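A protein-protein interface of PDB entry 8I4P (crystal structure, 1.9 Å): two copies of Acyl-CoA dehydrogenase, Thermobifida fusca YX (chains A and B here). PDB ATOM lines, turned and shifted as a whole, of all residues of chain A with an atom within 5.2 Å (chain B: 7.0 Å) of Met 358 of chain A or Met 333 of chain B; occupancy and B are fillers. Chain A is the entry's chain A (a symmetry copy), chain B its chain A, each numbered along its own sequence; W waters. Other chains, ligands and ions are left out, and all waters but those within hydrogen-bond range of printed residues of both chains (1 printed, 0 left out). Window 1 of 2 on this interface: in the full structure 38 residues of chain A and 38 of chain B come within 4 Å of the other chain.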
ATOM      1  N   MET A 333      -0.322  13.852   0.103  1.00  0.00           N
ATOM      2  CA  MET A 333      -0.347  14.938  -0.902  1.00  0.00           C
ATOM      3  C   MET A 333       0.980  15.031  -1.644  1.00  0.00           C
ATOM      4  O   MET A 333       0.956  15.129  -2.909  1.00  0.00           O
ATOM      5  CB  MET A 333      -0.657  16.267  -0.238  1.00  0.00           C
ATOM      6  CG  MET A 333      -1.155  17.311  -1.230  1.00  0.00           C
ATOM      7  SD  MET A 333      -2.691  16.898  -2.129  1.00  0.00           S
ATOM      8  CE  MET A 333      -2.070  16.363  -3.728  1.00  0.00           C
ATOM      9  N   THR A 336       1.619  11.599  -3.819  1.00  0.00           N
ATOM     10  CA  THR A 336       0.751  11.447  -5.010  1.00  0.00           C
ATOM     11  C   THR A 336       1.197  12.476  -6.040  1.00  0.00           C
ATOM     12  O   THR A 336       1.176  12.136  -7.226  1.00  0.00           O
ATOM     13  CB  THR A 336      -0.738  11.556  -4.704  1.00  0.00           C
ATOM     14  OG1 THR A 336      -0.948  12.816  -4.056  1.00  0.00           O
ATOM     15  CG2 THR A 336      -1.231  10.411  -3.848  1.00  0.00           C
ATOM     16  N   THR A 337       1.586  13.678  -5.623  1.00  0.00           N
ATOM     17  CA  THR A 337       2.057  14.720  -6.578  1.00  0.00           C
ATOM     18  C   THR A 337       3.340  14.215  -7.282  1.00  0.00           C
ATOM     19  O   THR A 337       3.480  14.398  -8.518  1.00  0.00           O
ATOM     20  CB  THR A 337       2.319  16.038  -5.842  1.00  0.00           C
ATOM     21  OG1 THR A 337       1.095  16.441  -5.244  1.00  0.00           O
ATOM     22  CG2 THR A 337       2.866  17.105  -6.737  1.00  0.00           C
ATOM     23  N   VAL A 340       2.533  11.216  -9.881  1.00  0.00           N
ATOM     24  CA  VAL A 340       2.131  11.750 -11.193  1.00  0.00           C
ATOM     25  C   VAL A 340       3.412  12.128 -11.947  1.00  0.00           C
ATOM     26  O   VAL A 340       3.560  11.754 -13.132  1.00  0.00           O
ATOM     27  CB  VAL A 340       1.195  12.947 -11.019  1.00  0.00           C
ATOM     28  CG1 VAL A 340       1.048  13.677 -12.335  1.00  0.00           C
ATOM     29  CG2 VAL A 340      -0.146  12.492 -10.477  1.00  0.00           C
ATOM     30  N   VAL A 354      -2.828   7.522 -11.228  1.00  0.00           N
ATOM     31  CA  VAL A 354      -2.031   8.326 -10.253  1.00  0.00           C
ATOM     32  C   VAL A 354      -2.612   9.740 -10.195  1.00  0.00           C
ATOM     33  O   VAL A 354      -2.711  10.227  -9.074  1.00  0.00           O
ATOM     34  CB  VAL A 354      -0.518   8.301 -10.466  1.00  0.00           C
ATOM     35  CG1 VAL A 354       0.040   6.920 -10.185  1.00  0.00           C
ATOM     36  CG2 VAL A 354      -0.099   8.833 -11.851  1.00  0.00           C
ATOM     37  N   GLU A 355      -3.160  10.293 -11.300  1.00  0.00           N
ATOM     38  CA  GLU A 355      -3.793  11.630 -11.214  1.00  0.00           C
ATOM     39  C   GLU A 355      -5.035  11.549 -10.309  1.00  0.00           C
ATOM     40  O   GLU A 355      -5.284  12.516  -9.562  1.00  0.00           O
ATOM     41  CB  GLU A 355      -4.023  12.267 -12.594  1.00  0.00           C
ATOM     42  CG  GLU A 355      -5.101  11.687 -13.486  1.00  0.00           C
ATOM     43  CD  GLU A 355      -6.540  11.989 -13.172  1.00  0.00           C
ATOM     44  OE1 GLU A 355      -7.366  11.054 -13.284  1.00  0.00           O
ATOM     45  OE2 GLU A 355      -6.825  13.162 -12.819  1.00  0.00           O
ATOM     46  N   ARG A 356      -5.828  10.477 -10.381  1.00  0.00           N
ATOM     47  CA  ARG A 356      -7.010  10.329  -9.479  1.00  0.00           C
ATOM     48  C   ARG A 356      -6.521  10.256  -8.022  1.00  0.00           C
ATOM     49  O   ARG A 356      -7.131  10.911  -7.087  1.00  0.00           O
ATOM     50  CB  ARG A 356      -7.872   9.112  -9.836  1.00  0.00           C
ATOM     51  CG  ARG A 356      -9.015   8.885  -8.852  1.00  0.00           C
ATOM     52  CD  ARG A 356      -9.608   7.519  -8.937  1.00  0.00           C
ATOM     53  NE  ARG A 356      -8.852   6.496  -8.291  1.00  0.00           N
ATOM     54  CZ  ARG A 356      -8.353   5.438  -8.883  1.00  0.00           C
ATOM     55  NH1 ARG A 356      -8.438   5.295 -10.201  1.00  0.00           N
ATOM     56  NH2 ARG A 356      -7.775   4.506  -8.138  1.00  0.00           N
ATOM     57  N   MET A 357      -5.457   9.506  -7.801  1.00  0.00           N
ATOM     58  CA  MET A 357      -4.879   9.327  -6.436  1.00  0.00           C
ATOM     59  C   MET A 357      -4.415  10.676  -5.893  1.00  0.00           C
ATOM     60  O   MET A 357      -4.704  10.962  -4.734  1.00  0.00           O
ATOM     61  CB  MET A 357      -3.769   8.289  -6.443  1.00  0.00           C
ATOM     62  CG  MET A 357      -4.312   6.886  -6.603  1.00  0.00           C
ATOM     63  SD  MET A 357      -2.942   5.828  -7.050  1.00  0.00           S
ATOM     64  CE  MET A 357      -3.645   4.197  -7.280  1.00  0.00           C
ATOM     65  N   MET A 358      -3.826  11.542  -6.733  1.00  0.00           N
ATOM     66  CA  MET A 358      -3.453  12.903  -6.296  1.00  0.00           C
ATOM     67  C   MET A 358      -4.690  13.752  -5.955  1.00  0.00           C
ATOM     68  O   MET A 358      -4.681  14.450  -4.871  1.00  0.00           O
ATOM     69  CB  MET A 358      -2.594  13.587  -7.362  1.00  0.00           C
ATOM     70  CG  MET A 358      -2.160  14.960  -6.972  1.00  0.00           C
ATOM     71  SD  MET A 358      -1.297  15.700  -8.422  1.00  0.00           S
ATOM     72  CE  MET A 358      -1.202  17.401  -7.875  1.00  0.00           C
ATOM     73  N   ARG A 359      -5.725  13.702  -6.796  1.00  0.00           N
ATOM     74  CA  ARG A 359      -6.978  14.484  -6.563  1.00  0.00           C
ATOM     75  C   ARG A 359      -7.636  13.983  -5.259  1.00  0.00           C
ATOM     76  O   ARG A 359      -8.108  14.810  -4.442  1.00  0.00           O
ATOM     77  CB  ARG A 359      -7.896  14.393  -7.781  1.00  0.00           C
ATOM     78  CG  ARG A 359      -7.316  15.010  -9.054  1.00  0.00           C
ATOM     79  CD  ARG A 359      -8.396  14.998 -10.146  1.00  0.00           C
ATOM     80  NE  ARG A 359      -8.501  13.721 -10.855  1.00  0.00           N
ATOM     81  CZ  ARG A 359      -9.544  12.874 -10.782  1.00  0.00           C
ATOM     82  NH1 ARG A 359     -10.543  13.093  -9.939  1.00  0.00           N
ATOM     83  NH2 ARG A 359      -9.561  11.778 -11.517  1.00  0.00           N
ATOM     84  N   ASP A 360      -7.594  12.673  -5.022  1.00  0.00           N
ATOM     85  CA  ASP A 360      -8.195  12.052  -3.796  1.00  0.00           C
ATOM     86  C   ASP A 360      -7.394  12.438  -2.546  1.00  0.00           C
ATOM     87  O   ASP A 360      -8.011  12.713  -1.498  1.00  0.00           O
ATOM     88  CB  ASP A 360      -8.274  10.533  -3.953  1.00  0.00           C
ATOM     89  CG  ASP A 360      -9.251  10.016  -5.035  1.00  0.00           C
ATOM     90  OD1 ASP A 360     -10.084  10.835  -5.602  1.00  0.00           O
ATOM     91  OD2 ASP A 360      -9.148   8.793  -5.343  1.00  0.00           O
ATOM     92  N   ALA A 361      -6.049  12.430  -2.626  1.00  0.00           N
ATOM     93  CA  ALA A 361      -5.146  12.703  -1.497  1.00  0.00           C
ATOM     94  C   ALA A 361      -5.506  14.077  -0.925  1.00  0.00           C
ATOM     95  O   ALA A 361      -5.537  14.190   0.311  1.00  0.00           O
ATOM     96  CB  ALA A 361      -3.693  12.579  -1.840  1.00  0.00           C
ATOM     97  N   LYS A 362      -5.870  15.035  -1.768  1.00  0.00           N
ATOM     98  CA  LYS A 362      -6.073  16.422  -1.287  1.00  0.00           C
ATOM     99  C   LYS A 362      -7.205  16.482  -0.249  1.00  0.00           C
ATOM    100  O   LYS A 362      -7.088  17.297   0.741  1.00  0.00           O
ATOM    101  CB  LYS A 362      -6.261  17.373  -2.470  1.00  0.00           C
ATOM    102  CG  LYS A 362      -6.568  18.801  -2.045  1.00  0.00           C
ATOM    103  CD  LYS A 362      -5.393  19.493  -1.413  1.00  0.00           C
ATOM    104  CE  LYS A 362      -5.766  20.391  -0.254  1.00  0.00           C
ATOM    105  NZ  LYS A 362      -4.567  20.989   0.367  1.00  0.00           N
ATOM    106  N   LEU B 206      -5.638  15.469 -16.328  1.00  0.00           N
ATOM    107  CA  LEU B 206      -5.906  16.017 -14.955  1.00  0.00           C
ATOM    108  C   LEU B 206      -6.351  17.473 -15.060  1.00  0.00           C
ATOM    109  O   LEU B 206      -7.337  17.859 -14.422  1.00  0.00           O
ATOM    110  CB  LEU B 206      -4.598  15.900 -14.184  1.00  0.00           C
ATOM    111  CG  LEU B 206      -4.499  16.618 -12.832  1.00  0.00           C
ATOM    112  CD1 LEU B 206      -5.598  16.144 -11.878  1.00  0.00           C
ATOM    113  CD2 LEU B 206      -3.120  16.328 -12.203  1.00  0.00           C
ATOM    114  N   ALA B 254       3.253  29.307 -15.029  1.00  0.00           N
ATOM    115  CA  ALA B 254       3.189  28.819 -13.634  1.00  0.00           C
ATOM    116  C   ALA B 254       2.972  29.991 -12.678  1.00  0.00           C
ATOM    117  O   ALA B 254       2.181  29.857 -11.724  1.00  0.00           O
ATOM    118  CB  ALA B 254       4.418  28.006 -13.273  1.00  0.00           C
ATOM    119  N   ALA B 258      -0.376  30.519 -10.257  1.00  0.00           N
ATOM    120  CA  ALA B 258      -0.158  30.693  -8.798  1.00  0.00           C
ATOM    121  C   ALA B 258      -0.745  32.028  -8.399  1.00  0.00           C
ATOM    122  O   ALA B 258      -1.361  32.125  -7.361  1.00  0.00           O
ATOM    123  CB  ALA B 258       1.321  30.639  -8.468  1.00  0.00           C
ATOM    124  N   PHE B 327      11.658  26.305 -10.826  1.00  0.00           N
ATOM    125  CA  PHE B 327      11.305  27.005  -9.582  1.00  0.00           C
ATOM    126  C   PHE B 327       9.840  27.423  -9.617  1.00  0.00           C
ATOM    127  O   PHE B 327       9.063  27.118  -8.636  1.00  0.00           O
ATOM    128  CB  PHE B 327      12.231  28.171  -9.279  1.00  0.00           C
ATOM    129  CG  PHE B 327      11.976  28.774  -7.927  1.00  0.00           C
ATOM    130  CD1 PHE B 327      12.309  28.101  -6.756  1.00  0.00           C
ATOM    131  CD2 PHE B 327      11.353  29.999  -7.824  1.00  0.00           C
ATOM    132  CE1 PHE B 327      12.055  28.680  -5.510  1.00  0.00           C
ATOM    133  CE2 PHE B 327      11.102  30.573  -6.577  1.00  0.00           C
ATOM    134  CZ  PHE B 327      11.450  29.906  -5.426  1.00  0.00           C
ATOM    135  N   ALA B 328       9.438  28.100 -10.689  1.00  0.00           N
ATOM    136  CA  ALA B 328       8.064  28.640 -10.791  1.00  0.00           C
ATOM    137  C   ALA B 328       7.011  27.539 -10.763  1.00  0.00           C
ATOM    138  O   ALA B 328       5.981  27.705 -10.077  1.00  0.00           O
ATOM    139  CB  ALA B 328       7.965  29.504 -11.996  1.00  0.00           C
ATOM    140  N   SER B 329       7.249  26.431 -11.467  1.00  0.00           N
ATOM    141  CA  SER B 329       6.263  25.338 -11.501  1.00  0.00           C
ATOM    142  C   SER B 329       6.192  24.643 -10.118  1.00  0.00           C
ATOM    143  O   SER B 329       5.053  24.354  -9.667  1.00  0.00           O
ATOM    144  CB  SER B 329       6.603  24.389 -12.627  1.00  0.00           C
ATOM    145  OG  SER B 329       7.920  23.937 -12.556  1.00  0.00           O
ATOM    146  N   ASP B 330       7.337  24.406  -9.450  1.00  0.00           N
ATOM    147  CA  ASP B 330       7.373  23.812  -8.087  1.00  0.00           C
ATOM    148  C   ASP B 330       6.573  24.720  -7.162  1.00  0.00           C
ATOM    149  O   ASP B 330       5.778  24.240  -6.403  1.00  0.00           O
ATOM    150  CB  ASP B 330       8.779  23.609  -7.528  1.00  0.00           C
ATOM    151  CG  ASP B 330       9.487  22.425  -8.169  1.00  0.00           C
ATOM    152  OD1 ASP B 330       8.820  21.642  -8.923  1.00  0.00           O
ATOM    153  OD2 ASP B 330      10.676  22.289  -7.933  1.00  0.00           O
ATOM    154  N   VAL B 331       6.832  26.007  -7.219  1.00  0.00           N
ATOM    155  CA  VAL B 331       6.143  27.013  -6.365  1.00  0.00           C
ATOM    156  C   VAL B 331       4.641  27.063  -6.700  1.00  0.00           C
ATOM    157  O   VAL B 331       3.763  27.172  -5.752  1.00  0.00           O
ATOM    158  CB  VAL B 331       6.887  28.351  -6.537  1.00  0.00           C
ATOM    159  CG1 VAL B 331       6.043  29.545  -6.141  1.00  0.00           C
ATOM    160  CG2 VAL B 331       8.190  28.294  -5.778  1.00  0.00           C
ATOM    161  N   ALA B 332       4.280  26.996  -7.977  1.00  0.00           N
ATOM    162  CA  ALA B 332       2.850  27.016  -8.362  1.00  0.00           C
ATOM    163  C   ALA B 332       2.147  25.750  -7.818  1.00  0.00           C
ATOM    164  O   ALA B 332       1.047  25.844  -7.335  1.00  0.00           O
ATOM    165  CB  ALA B 332       2.703  27.109  -9.857  1.00  0.00           C
ATOM    166  N   MET B 333       2.792  24.599  -7.906  1.00  0.00           N
ATOM    167  CA  MET B 333       2.205  23.365  -7.337  1.00  0.00           C
ATOM    168  C   MET B 333       1.927  23.525  -5.848  1.00  0.00           C
ATOM    169  O   MET B 333       0.800  23.150  -5.403  1.00  0.00           O
ATOM    170  CB  MET B 333       3.132  22.185  -7.562  1.00  0.00           C
ATOM    171  CG  MET B 333       2.413  20.848  -7.437  1.00  0.00           C
ATOM    172  SD  MET B 333       1.041  20.560  -8.608  1.00  0.00           S
ATOM    173  CE  MET B 333      -0.406  20.897  -7.598  1.00  0.00           C
ATOM    174  N   GLU B 334       2.894  24.060  -5.107  1.00  0.00           N
ATOM    175  CA  GLU B 334       2.730  24.254  -3.662  1.00  0.00           C
ATOM    176  C   GLU B 334       1.664  25.303  -3.424  1.00  0.00           C
ATOM    177  O   GLU B 334       0.848  25.078  -2.524  1.00  0.00           O
ATOM    178  CB  GLU B 334       3.991  24.706  -2.934  1.00  0.00           C
ATOM    179  CG  GLU B 334       5.086  23.664  -2.849  1.00  0.00           C
ATOM    180  CD  GLU B 334       6.489  24.210  -2.505  1.00  0.00           C
ATOM    181  OE1 GLU B 334       6.634  25.429  -2.067  1.00  0.00           O
ATOM    182  OE2 GLU B 334       7.438  23.435  -2.720  1.00  0.00           O
ATOM    183  N   ILE B 335       1.727  26.449  -4.086  1.00  0.00           N
ATOM    184  CA  ILE B 335       0.739  27.556  -3.823  1.00  0.00           C
ATOM    185  C   ILE B 335      -0.697  27.106  -4.135  1.00  0.00           C
ATOM    186  O   ILE B 335      -1.618  27.348  -3.287  1.00  0.00           O
ATOM    187  CB  ILE B 335       1.148  28.807  -4.616  1.00  0.00           C
ATOM    188  CG1 ILE B 335       2.382  29.473  -4.009  1.00  0.00           C
ATOM    189  CG2 ILE B 335       0.002  29.784  -4.743  1.00  0.00           C
ATOM    190  CD1 ILE B 335       2.945  30.564  -4.908  1.00  0.00           C
ATOM    191  N   THR B 336      -0.931  26.422  -5.254  1.00  0.00           N
ATOM    192  CA  THR B 336      -2.303  26.035  -5.657  1.00  0.00           C
ATOM    193  C   THR B 336      -2.800  24.994  -4.664  1.00  0.00           C
ATOM    194  O   THR B 336      -3.989  25.042  -4.340  1.00  0.00           O
ATOM    195  CB  THR B 336      -2.405  25.543  -7.096  1.00  0.00           C
ATOM    196  OG1 THR B 336      -1.485  24.453  -7.239  1.00  0.00           O
ATOM    197  CG2 THR B 336      -2.115  26.638  -8.097  1.00  0.00           C
ATOM    198  N   THR B 337      -1.942  24.092  -4.193  1.00  0.00           N
ATOM    199  CA  THR B 337      -2.359  23.064  -3.200  1.00  0.00           C
ATOM    200  C   THR B 337      -2.799  23.771  -1.895  1.00  0.00           C
ATOM    201  O   THR B 337      -3.828  23.374  -1.293  1.00  0.00           O
ATOM    202  CB  THR B 337      -1.211  22.085  -2.931  1.00  0.00           C
ATOM    203  OG1 THR B 337      -0.882  21.466  -4.167  1.00  0.00           O
ATOM    204  CG2 THR B 337      -1.545  21.069  -1.884  1.00  0.00           C
ATOM    205  N   ASP B 338      -2.107  24.845  -1.503  1.00  0.00           N
ATOM    206  CA  ASP B 338      -2.483  25.647  -0.313  1.00  0.00           C
ATOM    207  C   ASP B 338      -3.690  26.532  -0.569  1.00  0.00           C
ATOM    208  O   ASP B 338      -4.444  26.751   0.402  1.00  0.00           O
ATOM    209  CB  ASP B 338      -1.342  26.489   0.228  1.00  0.00           C
ATOM    210  CG  ASP B 338      -0.231  25.676   0.878  1.00  0.00           C
ATOM    211  OD1 ASP B 338      -0.460  24.522   1.290  1.00  0.00           O
ATOM    212  OD2 ASP B 338       0.850  26.208   0.957  1.00  0.00           O
ATOM    213  N   TYR B 348     -12.421  22.364  -2.424  1.00  0.00           N
ATOM    214  CA  TYR B 348     -12.409  21.004  -3.019  1.00  0.00           C
ATOM    215  C   TYR B 348     -13.538  20.896  -4.058  1.00  0.00           C
ATOM    216  O   TYR B 348     -13.682  19.790  -4.650  1.00  0.00           O
ATOM    217  CB  TYR B 348     -12.555  19.979  -1.883  1.00  0.00           C
ATOM    218  CG  TYR B 348     -12.070  18.622  -2.252  1.00  0.00           C
ATOM    219  CD1 TYR B 348     -10.709  18.366  -2.341  1.00  0.00           C
ATOM    220  CD2 TYR B 348     -12.942  17.580  -2.508  1.00  0.00           C
ATOM    221  CE1 TYR B 348     -10.223  17.115  -2.677  1.00  0.00           C
ATOM    222  CE2 TYR B 348     -12.464  16.313  -2.834  1.00  0.00           C
ATOM    223  CZ  TYR B 348     -11.109  16.073  -2.922  1.00  0.00           C
ATOM    224  OH  TYR B 348     -10.619  14.839  -3.275  1.00  0.00           O
ATOM    225  N   MET B 357      -7.165  25.308 -10.751  1.00  0.00           N
ATOM    226  CA  MET B 357      -5.817  25.951 -10.744  1.00  0.00           C
ATOM    227  C   MET B 357      -4.779  24.964 -10.217  1.00  0.00           C
ATOM    228  O   MET B 357      -3.717  24.864 -10.826  1.00  0.00           O
ATOM    229  CB  MET B 357      -5.835  27.252  -9.959  1.00  0.00           C
ATOM    230  CG  MET B 357      -6.563  28.349 -10.705  1.00  0.00           C
ATOM    231  SD  MET B 357      -6.916  29.652  -9.533  1.00  0.00           S
ATOM    232  CE  MET B 357      -7.823  30.896 -10.449  1.00  0.00           C
ATOM    233  N   MET B 358      -5.113  24.160  -9.196  1.00  0.00           N
ATOM    234  CA  MET B 358      -4.192  23.110  -8.712  1.00  0.00           C
ATOM    235  C   MET B 358      -3.964  22.019  -9.771  1.00  0.00           C
ATOM    236  O   MET B 358      -2.760  21.613  -9.991  1.00  0.00           O
ATOM    237  CB  MET B 358      -4.713  22.508  -7.405  1.00  0.00           C
ATOM    238  CG  MET B 358      -3.815  21.456  -6.846  1.00  0.00           C
ATOM    239  SD  MET B 358      -4.667  20.719  -5.388  1.00  0.00           S
ATOM    240  CE  MET B 358      -3.619  19.293  -5.121  1.00  0.00           C
ATOM    241  N   ARG B 359      -5.033  21.562 -10.428  1.00  0.00           N
ATOM    242  CA  ARG B 359      -4.928  20.502 -11.479  1.00  0.00           C
ATOM    243  C   ARG B 359      -4.078  21.050 -12.646  1.00  0.00           C
ATOM    244  O   ARG B 359      -3.211  20.318 -13.182  1.00  0.00           O
ATOM    245  CB  ARG B 359      -6.318  20.037 -11.905  1.00  0.00           C
ATOM    246  CG  ARG B 359      -7.126  19.366 -10.795  1.00  0.00           C
ATOM    247  CD  ARG B 359      -8.424  18.805 -11.395  1.00  0.00           C
ATOM    248  NE  ARG B 359      -9.491  19.799 -11.521  1.00  0.00           N
ATOM    249  CZ  ARG B 359      -9.975  20.278 -12.682  1.00  0.00           C
ATOM    250  NH1 ARG B 359      -9.418  19.953 -13.840  1.00  0.00           N
ATOM    251  NH2 ARG B 359     -10.987  21.126 -12.679  1.00  0.00           N
ATOM    252  N   ASP B 360      -4.254  22.328 -12.979  1.00  0.00           N
ATOM    253  CA  ASP B 360      -3.497  22.987 -14.093  1.00  0.00           C
ATOM    254  C   ASP B 360      -2.018  23.150 -13.719  1.00  0.00           C
ATOM    255  O   ASP B 360      -1.151  22.935 -14.590  1.00  0.00           O
ATOM    256  CB  ASP B 360      -4.129  24.334 -14.443  1.00  0.00           C
ATOM    257  CG  ASP B 360      -5.545  24.275 -15.065  1.00  0.00           C
ATOM    258  OD1 ASP B 360      -6.039  23.136 -15.443  1.00  0.00           O
ATOM    259  OD2 ASP B 360      -6.172  25.371 -15.131  1.00  0.00           O
ATOM    260  N   ALA B 361      -1.720  23.554 -12.469  1.00  0.00           N
ATOM    261  CA  ALA B 361      -0.358  23.826 -11.985  1.00  0.00           C
ATOM    262  C   ALA B 361       0.486  22.569 -12.212  1.00  0.00           C
ATOM    263  O   ALA B 361       1.637  22.726 -12.651  1.00  0.00           O
ATOM    264  CB  ALA B 361      -0.305  24.314 -10.569  1.00  0.00           C
ATOM    265  N   LYS B 362      -0.087  21.385 -12.037  1.00  0.00           N
ATOM    266  CA  LYS B 362       0.721  20.144 -12.087  1.00  0.00           C
ATOM    267  C   LYS B 362       1.370  19.968 -13.469  1.00  0.00           C
ATOM    268  O   LYS B 362       2.554  19.467 -13.532  1.00  0.00           O
ATOM    269  CB  LYS B 362      -0.114  18.946 -11.633  1.00  0.00           C
ATOM    270  CG  LYS B 362       0.627  17.623 -11.749  1.00  0.00           C
ATOM    271  CD  LYS B 362       1.741  17.483 -10.750  1.00  0.00           C
ATOM    272  CE  LYS B 362       2.969  16.790 -11.300  1.00  0.00           C
ATOM    273  NZ  LYS B 362       4.051  16.742 -10.297  1.00  0.00           N
ATOM    274  N   ILE B 363       0.727  20.419 -14.554  1.00  0.00           N
ATOM    275  CA  ILE B 363       1.338  20.220 -15.916  1.00  0.00           C
ATOM    276  C   ILE B 363       2.652  20.992 -16.025  1.00  0.00           C
ATOM    277  O   ILE B 363       3.564  20.539 -16.765  1.00  0.00           O
ATOM    278  CB  ILE B 363       0.380  20.548 -17.088  1.00  0.00           C
ATOM    279  CG1 ILE B 363       0.963  20.036 -18.417  1.00  0.00           C
ATOM    280  CG2 ILE B 363       0.078  22.040 -17.206  1.00  0.00           C
ATOM    281  CD1 ILE B 363       1.311  18.558 -18.458  1.00  0.00           C
ATOM    282  N   THR B 364       2.769  22.150 -15.374  1.00  0.00           N
ATOM    283  CA  THR B 364       3.941  23.050 -15.517  1.00  0.00           C
ATOM    284  C   THR B 364       5.221  22.359 -15.021  1.00  0.00           C
ATOM    285  O   THR B 364       6.299  22.754 -15.482  1.00  0.00           O
ATOM    286  CB  THR B 364       3.723  24.399 -14.837  1.00  0.00           C
ATOM    287  OG1 THR B 364       3.677  24.301 -13.421  1.00  0.00           O
ATOM    288  CG2 THR B 364       2.449  25.025 -15.340  1.00  0.00           C
ATOM    289  N   GLN B 365       5.105  21.357 -14.133  1.00  0.00           N
ATOM    290  CA  GLN B 365       6.272  20.571 -13.641  1.00  0.00           C
ATOM    291  C   GLN B 365       6.694  19.517 -14.667  1.00  0.00           C
ATOM    292  O   GLN B 365       7.810  18.959 -14.520  1.00  0.00           O
ATOM    293  CB  GLN B 365       5.924  19.888 -12.314  1.00  0.00           C
ATOM    294  CG  GLN B 365       5.594  20.870 -11.215  1.00  0.00           C
ATOM    295  CD  GLN B 365       5.344  20.135  -9.919  1.00  0.00           C
ATOM    296  OE1 GLN B 365       4.352  19.463  -9.750  1.00  0.00           O
ATOM    297  NE2 GLN B 365       6.237  20.309  -8.977  1.00  0.00           N
HETATM  298  O   HOH W   1      -2.132  22.283   1.741  1.00  0.00           O
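Met 333 of chain A touches Thr 337 of chain B, and with the chains exchanged Thr 337 of chain A touches Met 333 of chain B.
Met 333 of chain A touches Met 358 of chain B, and with the chains exchanged Met 358 of chain A touches Met 333 of chain B.
Thr 337 of chain A touches Lys 362 of chain B, and with the chains exchanged Lys 362 of chain A touches Thr 337 of chain B.
9 positions are printed for both chains.
Of the 25 printed residues of chain B, 6 touch a printed residue of chain A.
Hydrophobic or aromatic side chains of chain B that line the printed part of chain A: Leu 206, Met 333, Tyr 348 and Met 358.
Among the printed residues, 12 pairs touch across the chains.
Water W1 bridges the side-chain carboxylate (OD1) of Asp 338 of chain B and the side-chain amino group (NZ) of Lys 362 of chain A.
O of Thr 337 of chain B lies within hydrogen-bond range of NZ of Lys 362 of chain A, 3.0 Å away.
OH of Tyr 348 of chain B sits at hydrogen-bond distance from O of Arg 359 of chain A (2.8 Å).
The side-chain amino group (NZ) of Lys 362 of chain B lies within hydrogen-bond range of the backbone carbonyl oxygen (O) of Thr 337 of chain A.
Of the printed residues of chain B, Glu 355 of chain A touches Leu 206.
Of chain B, only Met 333 comes within 4 Å of Met 358 of chain A.
Of the printed residues of chain A, Leu 206 of chain B touches Glu 355 (3.4 Å) and Arg 359 (3.5 Å).
Met 333 of chain B touches two residues of chain A.
Printed residues of chain A within 4 Å of Tyr 348 of chain B: Arg 359 (2.8 Å), Asp 360 (3.7 Å) and Lys 362 (3.9 Å).
Arg 359 of chain B touches none of the printed residues of chain A.
CG of Met 333 of chain A touches CG2 of Thr 337 of chain B, 3.8 Å away.
CE of Met 333 of chain A touches CE of Met 358 of chain B, 3.6 Å away.
Met 333 of chain B touches Thr 337 of chain A (CG to CG2, 3.8 Å).
Val 340 of chain A touches Lys 362 of chain B (CG1 to CE, 3.8 Å).
Glu 355 of chain A touches Leu 206 of chain B (OE2 to CD1, 3.4 Å).
Met 333 of chain B touches Met 358 of chain A (CE to CE, 3.6 Å).
Leu 206 of chain B touches Arg 359 of chain A (CD1 to CD, 3.5 Å).
Tyr 348 of chain B touches Asp 360 of chain A (OH to CA, 3.7 Å).
C of Lys 362 of chain A touches CE1 of Tyr 348 of chain B, at 3.9 Å.
The backbone carbonyl oxygen (O) of Leu 206 of chain B is in hydrogen-bond range of the guanidinium group (NH1) of Arg 359 of chain B.
N of Lys 362 of chain B sits close to SD of Met 333 of chain B (3.7 Å).
The side-chain amide oxygen (OE1) of Gln 365 of chain B sits close to the side-chain sulfur (SD) of Met 333 of chain B, at 3.7 Å.
O of Met 333 of chain A sits at hydrogen-bond distance from OG1 of Thr 336 of chain A (3.2 Å).
O of Met 333 of chain A lies within hydrogen-bond range of OG1 of Thr 337 of chain A (2.7 Å).
The guanidinium group (NE) of Arg 356 of chain A lies within salt-bridge range of the side-chain carboxylate (OD2) of Asp 360 of chain A, at 3.7 Å.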
